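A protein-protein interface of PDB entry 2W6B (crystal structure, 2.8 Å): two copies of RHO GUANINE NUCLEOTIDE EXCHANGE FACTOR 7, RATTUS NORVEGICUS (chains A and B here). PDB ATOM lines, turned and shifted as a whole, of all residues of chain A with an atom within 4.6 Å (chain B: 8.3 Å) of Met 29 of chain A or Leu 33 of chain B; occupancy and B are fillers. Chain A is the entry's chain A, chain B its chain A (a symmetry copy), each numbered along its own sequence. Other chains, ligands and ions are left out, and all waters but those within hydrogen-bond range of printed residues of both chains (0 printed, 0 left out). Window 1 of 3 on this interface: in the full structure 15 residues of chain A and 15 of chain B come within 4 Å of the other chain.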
ATOM      1  N   ASP A  25     -27.474   8.172   8.326  1.00  0.00           N
ATOM      2  CA  ASP A  25     -27.521   8.179   6.874  1.00  0.00           C
ATOM      3  C   ASP A  25     -26.236   8.705   6.247  1.00  0.00           C
ATOM      4  O   ASP A  25     -25.795   8.189   5.221  1.00  0.00           O
ATOM      5  CB  ASP A  25     -28.741   8.956   6.375  1.00  0.00           C
ATOM      6  CG  ASP A  25     -30.055   8.170   6.531  1.00  0.00           C
ATOM      7  OD1 ASP A  25     -30.049   6.905   6.547  1.00  0.00           O
ATOM      8  OD2 ASP A  25     -31.111   8.834   6.629  1.00  0.00           O
ATOM      9  N   ASN A  26     -25.639   9.724   6.857  1.00  0.00           N
ATOM     10  CA  ASN A  26     -24.291  10.117   6.500  1.00  0.00           C
ATOM     11  C   ASN A  26     -23.346   8.935   6.544  1.00  0.00           C
ATOM     12  O   ASN A  26     -22.683   8.619   5.559  1.00  0.00           O
ATOM     13  CB  ASN A  26     -23.794  11.180   7.455  1.00  0.00           C
ATOM     14  CG  ASN A  26     -24.298  12.549   7.095  1.00  0.00           C
ATOM     15  OD1 ASN A  26     -25.341  12.697   6.443  1.00  0.00           O
ATOM     16  ND2 ASN A  26     -23.558  13.570   7.511  1.00  0.00           N
ATOM     17  N   LYS A  27     -23.310   8.279   7.700  1.00  0.00           N
ATOM     18  CA  LYS A  27     -22.510   7.080   7.901  1.00  0.00           C
ATOM     19  C   LYS A  27     -22.559   6.195   6.663  1.00  0.00           C
ATOM     20  O   LYS A  27     -21.530   5.958   6.034  1.00  0.00           O
ATOM     21  CB  LYS A  27     -22.956   6.345   9.187  1.00  0.00           C
ATOM     22  CG  LYS A  27     -22.616   4.840   9.280  1.00  0.00           C
ATOM     23  CD  LYS A  27     -23.872   3.948   9.149  1.00  0.00           C
ATOM     24  CE  LYS A  27     -23.524   2.547   8.655  1.00  0.00           C
ATOM     25  NZ  LYS A  27     -22.385   1.947   9.418  1.00  0.00           N
ATOM     26  N   LYS A  28     -23.753   5.745   6.286  1.00  0.00           N
ATOM     27  CA  LYS A  28     -23.850   4.833   5.157  1.00  0.00           C
ATOM     28  C   LYS A  28     -23.643   5.519   3.814  1.00  0.00           C
ATOM     29  O   LYS A  28     -23.288   4.867   2.841  1.00  0.00           O
ATOM     30  CB  LYS A  28     -25.102   3.931   5.193  1.00  0.00           C
ATOM     31  CG  LYS A  28     -26.468   4.602   5.198  1.00  0.00           C
ATOM     32  CD  LYS A  28     -27.557   3.567   4.838  1.00  0.00           C
ATOM     33  CE  LYS A  28     -28.670   3.491   5.904  1.00  0.00           C
ATOM     34  NZ  LYS A  28     -28.206   2.836   7.187  1.00  0.00           N
ATOM     35  N   MET A  29     -23.829   6.828   3.758  1.00  0.00           N
ATOM     36  CA  MET A  29     -23.605   7.523   2.509  1.00  0.00           C
ATOM     37  C   MET A  29     -22.129   7.645   2.259  1.00  0.00           C
ATOM     38  O   MET A  29     -21.650   7.365   1.168  1.00  0.00           O
ATOM     39  CB  MET A  29     -24.213   8.901   2.556  1.00  0.00           C
ATOM     40  CG  MET A  29     -24.525   9.422   1.190  1.00  0.00           C
ATOM     41  SD  MET A  29     -26.187  10.408   1.285  1.00  0.00           S
ATOM     42  CE  MET A  29     -27.437   8.989   1.839  1.00  0.00           C
ATOM     43  N   LYS A  30     -21.418   8.083   3.291  1.00  0.00           N
ATOM     44  CA  LYS A  30     -19.982   8.121   3.287  1.00  0.00           C
ATOM     45  C   LYS A  30     -19.519   6.762   2.816  1.00  0.00           C
ATOM     46  O   LYS A  30     -18.595   6.656   2.032  1.00  0.00           O
ATOM     47  CB  LYS A  30     -19.484   8.421   4.703  1.00  0.00           C
ATOM     48  CG  LYS A  30     -17.981   8.603   4.833  1.00  0.00           C
ATOM     49  CD  LYS A  30     -17.605   9.801   5.724  1.00  0.00           C
ATOM     50  CE  LYS A  30     -16.085  10.010   5.728  1.00  0.00           C
ATOM     51  NZ  LYS A  30     -15.717  11.416   6.077  1.00  0.00           N
ATOM     52  N   LYS A  31     -20.226   5.730   3.263  1.00  0.00           N
ATOM     53  CA  LYS A  31     -19.865   4.340   3.027  1.00  0.00           C
ATOM     54  C   LYS A  31     -19.938   3.942   1.553  1.00  0.00           C
ATOM     55  O   LYS A  31     -19.016   3.332   1.031  1.00  0.00           O
ATOM     56  CB  LYS A  31     -20.763   3.433   3.881  1.00  0.00           C
ATOM     57  CG  LYS A  31     -20.252   2.023   4.160  1.00  0.00           C
ATOM     58  CD  LYS A  31     -21.368   1.189   4.800  1.00  0.00           C
ATOM     59  CE  LYS A  31     -20.956  -0.271   5.027  1.00  0.00           C
ATOM     60  NZ  LYS A  31     -20.200  -0.511   6.300  1.00  0.00           N
ATOM     61  N   SER A  32     -21.024   4.289   0.880  1.00  0.00           N
ATOM     62  CA  SER A  32     -21.254   3.806  -0.486  1.00  0.00           C
ATOM     63  C   SER A  32     -20.725   4.759  -1.540  1.00  0.00           C
ATOM     64  O   SER A  32     -20.596   4.408  -2.708  1.00  0.00           O
ATOM     65  CB  SER A  32     -22.737   3.588  -0.723  1.00  0.00           C
ATOM     66  OG  SER A  32     -23.372   4.838  -0.859  1.00  0.00           O
ATOM     67  N   LEU A  33     -20.463   5.987  -1.125  1.00  0.00           N
ATOM     68  CA  LEU A  33     -19.680   6.893  -1.917  1.00  0.00           C
ATOM     69  C   LEU A  33     -18.310   6.252  -2.037  1.00  0.00           C
ATOM     70  O   LEU A  33     -17.755   6.159  -3.127  1.00  0.00           O
ATOM     71  CB  LEU A  33     -19.557   8.217  -1.187  1.00  0.00           C
ATOM     72  CG  LEU A  33     -19.526   9.494  -2.011  1.00  0.00           C
ATOM     73  CD1 LEU A  33     -19.297  10.642  -1.048  1.00  0.00           C
ATOM     74  CD2 LEU A  33     -18.455   9.467  -3.118  1.00  0.00           C
ATOM     75  N   ASP B  25     -31.573  17.525   1.624  1.00  0.00           N
ATOM     76  CA  ASP B  25     -30.313  17.383   0.916  1.00  0.00           C
ATOM     77  C   ASP B  25     -29.840  15.937   0.842  1.00  0.00           C
ATOM     78  O   ASP B  25     -29.299  15.517  -0.181  1.00  0.00           O
ATOM     79  CB  ASP B  25     -29.242  18.285   1.532  1.00  0.00           C
ATOM     80  CG  ASP B  25     -29.421  19.768   1.156  1.00  0.00           C
ATOM     81  OD1 ASP B  25     -30.010  20.092   0.084  1.00  0.00           O
ATOM     82  OD2 ASP B  25     -28.953  20.619   1.944  1.00  0.00           O
ATOM     83  N   ASN B  26     -30.043  15.178   1.915  1.00  0.00           N
ATOM     84  CA  ASN B  26     -29.877  13.741   1.850  1.00  0.00           C
ATOM     85  C   ASN B  26     -30.676  13.149   0.709  1.00  0.00           C
ATOM     86  O   ASN B  26     -30.132  12.470  -0.159  1.00  0.00           O
ATOM     87  CB  ASN B  26     -30.332  13.111   3.148  1.00  0.00           C
ATOM     88  CG  ASN B  26     -29.282  13.193   4.220  1.00  0.00           C
ATOM     89  OD1 ASN B  26     -28.406  14.070   4.194  1.00  0.00           O
ATOM     90  ND2 ASN B  26     -29.350  12.272   5.174  1.00  0.00           N
ATOM     91  N   LYS B  27     -31.975  13.431   0.718  1.00  0.00           N
ATOM     92  CA  LYS B  27     -32.883  13.002  -0.336  1.00  0.00           C
ATOM     93  C   LYS B  27     -32.211  13.120  -1.696  1.00  0.00           C
ATOM     94  O   LYS B  27     -32.022  12.116  -2.381  1.00  0.00           O
ATOM     95  CB  LYS B  27     -34.215  13.783  -0.251  1.00  0.00           C
ATOM     96  CG  LYS B  27     -35.059  13.859  -1.543  1.00  0.00           C
ATOM     97  CD  LYS B  27     -35.055  15.276  -2.161  1.00  0.00           C
ATOM     98  CE  LYS B  27     -35.350  15.243  -3.657  1.00  0.00           C
ATOM     99  NZ  LYS B  27     -36.547  14.406  -3.978  1.00  0.00           N
ATOM    100  N   LYS B  28     -31.808  14.332  -2.070  1.00  0.00           N
ATOM    101  CA  LYS B  28     -31.230  14.517  -3.392  1.00  0.00           C
ATOM    102  C   LYS B  28     -29.814  13.970  -3.509  1.00  0.00           C
ATOM    103  O   LYS B  28     -29.359  13.675  -4.606  1.00  0.00           O
ATOM    104  CB  LYS B  28     -31.373  15.954  -3.936  1.00  0.00           C
ATOM    105  CG  LYS B  28     -30.749  17.089  -3.138  1.00  0.00           C
ATOM    106  CD  LYS B  28     -30.650  18.354  -4.019  1.00  0.00           C
ATOM    107  CE  LYS B  28     -31.338  19.575  -3.372  1.00  0.00           C
ATOM    108  NZ  LYS B  28     -32.847  19.464  -3.369  1.00  0.00           N
ATOM    109  N   MET B  29     -29.127  13.801  -2.390  1.00  0.00           N
ATOM    110  CA  MET B  29     -27.793  13.249  -2.455  1.00  0.00           C
ATOM    111  C   MET B  29     -27.872  11.771  -2.718  1.00  0.00           C
ATOM    112  O   MET B  29     -27.176  11.246  -3.577  1.00  0.00           O
ATOM    113  CB  MET B  29     -27.062  13.479  -1.158  1.00  0.00           C
ATOM    114  CG  MET B  29     -25.578  13.469  -1.341  1.00  0.00           C
ATOM    115  SD  MET B  29     -24.817  14.816  -0.179  1.00  0.00           S
ATOM    116  CE  MET B  29     -25.642  16.452  -0.907  1.00  0.00           C
ATOM    117  N   LYS B  30     -28.728  11.109  -1.950  1.00  0.00           N
ATOM    118  CA  LYS B  30     -29.048   9.723  -2.156  1.00  0.00           C
ATOM    119  C   LYS B  30     -29.371   9.573  -3.624  1.00  0.00           C
ATOM    120  O   LYS B  30     -28.965   8.616  -4.256  1.00  0.00           O
ATOM    121  CB  LYS B  30     -30.245   9.349  -1.279  1.00  0.00           C
ATOM    122  CG  LYS B  30     -30.631   7.880  -1.307  1.00  0.00           C
ATOM    123  CD  LYS B  30     -30.941   7.323   0.094  1.00  0.00           C
ATOM    124  CE  LYS B  30     -31.210   5.814   0.025  1.00  0.00           C
ATOM    125  NZ  LYS B  30     -30.958   5.142   1.335  1.00  0.00           N
ATOM    126  N   LYS B  31     -30.056  10.574  -4.165  1.00  0.00           N
ATOM    127  CA  LYS B  31     -30.570  10.558  -5.526  1.00  0.00           C
ATOM    128  C   LYS B  31     -29.468  10.543  -6.585  1.00  0.00           C
ATOM    129  O   LYS B  31     -29.515   9.753  -7.517  1.00  0.00           O
ATOM    130  CB  LYS B  31     -31.503  11.762  -5.728  1.00  0.00           C
ATOM    131  CG  LYS B  31     -32.505  11.674  -6.875  1.00  0.00           C
ATOM    132  CD  LYS B  31     -33.168  13.040  -7.084  1.00  0.00           C
ATOM    133  CE  LYS B  31     -34.124  13.053  -8.284  1.00  0.00           C
ATOM    134  NZ  LYS B  31     -35.506  12.553  -7.981  1.00  0.00           N
ATOM    135  N   SER B  32     -28.476  11.408  -6.445  1.00  0.00           N
ATOM    136  CA  SER B  32     -27.467  11.579  -7.497  1.00  0.00           C
ATOM    137  C   SER B  32     -26.255  10.692  -7.295  1.00  0.00           C
ATOM    138  O   SER B  32     -25.442  10.510  -8.196  1.00  0.00           O
ATOM    139  CB  SER B  32     -27.011  13.025  -7.557  1.00  0.00           C
ATOM    140  OG  SER B  32     -26.175  13.292  -6.454  1.00  0.00           O
ATOM    141  N   LEU B  33     -26.115  10.175  -6.085  1.00  0.00           N
ATOM    142  CA  LEU B  33     -25.209   9.090  -5.836  1.00  0.00           C
ATOM    143  C   LEU B  33     -25.723   7.929  -6.667  1.00  0.00           C
ATOM    144  O   LEU B  33     -24.960   7.283  -7.379  1.00  0.00           O
ATOM    145  CB  LEU B  33     -25.263   8.722  -4.365  1.00  0.00           C
ATOM    146  CG  LEU B  33     -23.983   8.256  -3.691  1.00  0.00           C
ATOM    147  CD1 LEU B  33     -24.343   7.862  -2.273  1.00  0.00           C
ATOM    148  CD2 LEU B  33     -23.299   7.098  -4.440  1.00  0.00           C
ATOM    149  N   GLU B  34     -27.033   7.695  -6.596  1.00  0.00           N
ATOM    150  CA  GLU B  34     -27.680   6.618  -7.328  1.00  0.00           C
ATOM    151  C   GLU B  34     -27.630   6.788  -8.839  1.00  0.00           C
ATOM    152  O   GLU B  34     -27.522   5.801  -9.547  1.00  0.00           O
ATOM    153  CB  GLU B  34     -29.112   6.413  -6.837  1.00  0.00           C
ATOM    154  CG  GLU B  34     -29.198   5.557  -5.562  1.00  0.00           C
ATOM    155  CD  GLU B  34     -30.584   5.556  -4.906  1.00  0.00           C
ATOM    156  OE1 GLU B  34     -31.487   6.280  -5.399  1.00  0.00           O
ATOM    157  OE2 GLU B  34     -30.768   4.830  -3.888  1.00  0.00           O
ATOM    158  N   GLU B  35     -27.696   8.023  -9.334  1.00  0.00           N
ATOM    159  CA  GLU B  35     -27.474   8.295 -10.766  1.00  0.00           C
ATOM    160  C   GLU B  35     -26.038   7.997 -11.229  1.00  0.00           C
ATOM    161  O   GLU B  35     -25.803   7.625 -12.380  1.00  0.00           O
ATOM    162  CB  GLU B  35     -27.839   9.743 -11.119  1.00  0.00           C
ATOM    163  CG  GLU B  35     -29.203   9.911 -11.813  1.00  0.00           C
ATOM    164  CD  GLU B  35     -30.298  10.488 -10.905  1.00  0.00           C
ATOM    165  OE1 GLU B  35     -31.240   9.739 -10.526  1.00  0.00           O
ATOM    166  OE2 GLU B  35     -30.221  11.702 -10.588  1.00  0.00           O
ATOM    167  N   GLU B  36     -25.091   8.164 -10.313  1.00  0.00           N
ATOM    168  CA  GLU B  36     -23.667   7.972 -10.565  1.00  0.00           C
ATOM    169  C   GLU B  36     -23.330   6.494 -10.700  1.00  0.00           C
ATOM    170  O   GLU B  36     -22.611   6.109 -11.598  1.00  0.00           O
ATOM    171  CB  GLU B  36     -22.875   8.619  -9.419  1.00  0.00           C
ATOM    172  CG  GLU B  36     -21.379   8.811  -9.637  1.00  0.00           C
ATOM    173  CD  GLU B  36     -21.042   9.408 -10.989  1.00  0.00           C
ATOM    174  OE1 GLU B  36     -20.126   8.867 -11.645  1.00  0.00           O
ATOM    175  OE2 GLU B  36     -21.691  10.398 -11.404  1.00  0.00           O
ATOM    176  N   GLN B  37     -23.864   5.677  -9.802  1.00  0.00           N
ATOM    177  CA  GLN B  37     -23.748   4.226  -9.889  1.00  0.00           C
ATOM    178  C   GLN B  37     -24.168   3.737 -11.261  1.00  0.00           C
ATOM    179  O   GLN B  37     -23.467   2.948 -11.886  1.00  0.00           O
ATOM    180  CB  GLN B  37     -24.661   3.550  -8.866  1.00  0.00           C
ATOM    181  CG  GLN B  37     -24.249   3.684  -7.406  1.00  0.00           C
ATOM    182  CD  GLN B  37     -25.178   2.920  -6.471  1.00  0.00           C
ATOM    183  OE1 GLN B  37     -25.774   1.904  -6.855  1.00  0.00           O
ATOM    184  NE2 GLN B  37     -25.310   3.404  -5.235  1.00  0.00           N
ATOM    185  N   ARG B  38     -25.329   4.211 -11.709  1.00  0.00           N
ATOM    186  CA  ARG B  38     -25.936   3.819 -12.982  1.00  0.00           C
ATOM    187  C   ARG B  38     -25.076   4.294 -14.149  1.00  0.00           C
ATOM    188  O   ARG B  38     -24.803   3.535 -15.081  1.00  0.00           O
ATOM    189  CB  ARG B  38     -27.377   4.371 -13.066  1.00  0.00           C
ATOM    190  CG  ARG B  38     -28.084   4.289 -14.431  1.00  0.00           C
ATOM    191  CD  ARG B  38     -29.632   4.363 -14.301  1.00  0.00           C
ATOM    192  NE  ARG B  38     -30.282   5.685 -14.109  1.00  0.00           N
ATOM    193  CZ  ARG B  38     -29.792   6.903 -14.403  1.00  0.00           C
ATOM    194  NH1 ARG B  38     -28.578   7.076 -14.930  1.00  0.00           N
ATOM    195  NH2 ARG B  38     -30.545   7.977 -14.166  1.00  0.00           N
ATOM    196  N   ALA B  39     -24.630   5.541 -14.080  1.00  0.00           N
ATOM    197  CA  ALA B  39     -23.781   6.082 -15.120  1.00  0.00           C
ATOM    198  C   ALA B  39     -22.500   5.268 -15.302  1.00  0.00           C
ATOM    199  O   ALA B  39     -22.038   5.086 -16.428  1.00  0.00           O
ATOM    200  CB  ALA B  39     -23.458   7.498 -14.822  1.00  0.00           C
ATOM    201  N   ARG B  40     -21.932   4.766 -14.206  1.00  0.00           N
ATOM    202  CA  ARG B  40     -20.679   4.032 -14.305  1.00  0.00           C
ATOM    203  C   ARG B  40     -20.890   2.560 -14.574  1.00  0.00           C
ATOM    204  O   ARG B  40     -20.073   1.944 -15.248  1.00  0.00           O
ATOM    205  CB  ARG B  40     -19.756   4.285 -13.104  1.00  0.00           C
ATOM    206  CG  ARG B  40     -19.878   3.328 -11.955  1.00  0.00           C
ATOM    207  CD  ARG B  40     -18.768   2.287 -11.897  1.00  0.00           C
ATOM    208  NE  ARG B  40     -18.911   1.507 -10.666  1.00  0.00           N
ATOM    209  CZ  ARG B  40     -19.709   0.449 -10.523  1.00  0.00           C
ATOM    210  NH1 ARG B  40     -20.423   0.006 -11.546  1.00  0.00           N
ATOM    211  NH2 ARG B  40     -19.793  -0.181  -9.356  1.00  0.00           N
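Asn 26 of chain B touches Asp 25 of chain A (ND2 to CB, 3.6 Å). Met 29 of chain A touches Leu 33 of chain B (CG to CD1, 3.8 Å). Ser 32 of chain A touches Leu 33 of chain B (OG to CD1, 3.5 Å).
Of the printed residues of chain B, Asp 25 of chain A touches Asn 26 (3.6 Å). Lys 28 of chain A touches none of the printed residues of chain B. Of chain B, only Leu 33 comes within 4 Å of Met 29 of chain A. Printed residues of chain B within 4 Å of Ser 32 of chain A: Leu 33 (3.5 Å). Asp 25 of chain B touches none of the printed residues of chain A. Printed residues of chain A within 4 Å of Asn 26 of chain B: Asp 25. Leu 33 of chain B touches two residues of chain A. The nearest residue of chain B that does not touch Met 29 of chain A is Met 29 of chain B (4.02 Å). The nearest residue of chain A that does not touch Leu 33 of chain B is Leu 33 of chain A (4.4 Å).
Hydrophobic or aromatic side chains of chain A within 4 Å of the printed part of chain B: Met 29. Among the printed residues, no Asp or Glu carboxylate lies within 4 Å of a Lys or Arg side-chain nitrogen of the other chain.
Asp 25 of chain A touches Asn 26 of chain B, but with the chains exchanged Asn 26 of chain A does not touch Asp 25 of chain B (7.9 Å). Met 29 of chain A touches Leu 33 of chain B, but with the chains exchanged Leu 33 of chain A does not touch Met 29 of chain B (6.9 Å). Ser 32 of chain A touches Leu 33 of chain B, but with the chains exchanged Leu 33 of chain A does not touch Ser 32 of chain B (8.6 Å). 9 positions are printed for both chains.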
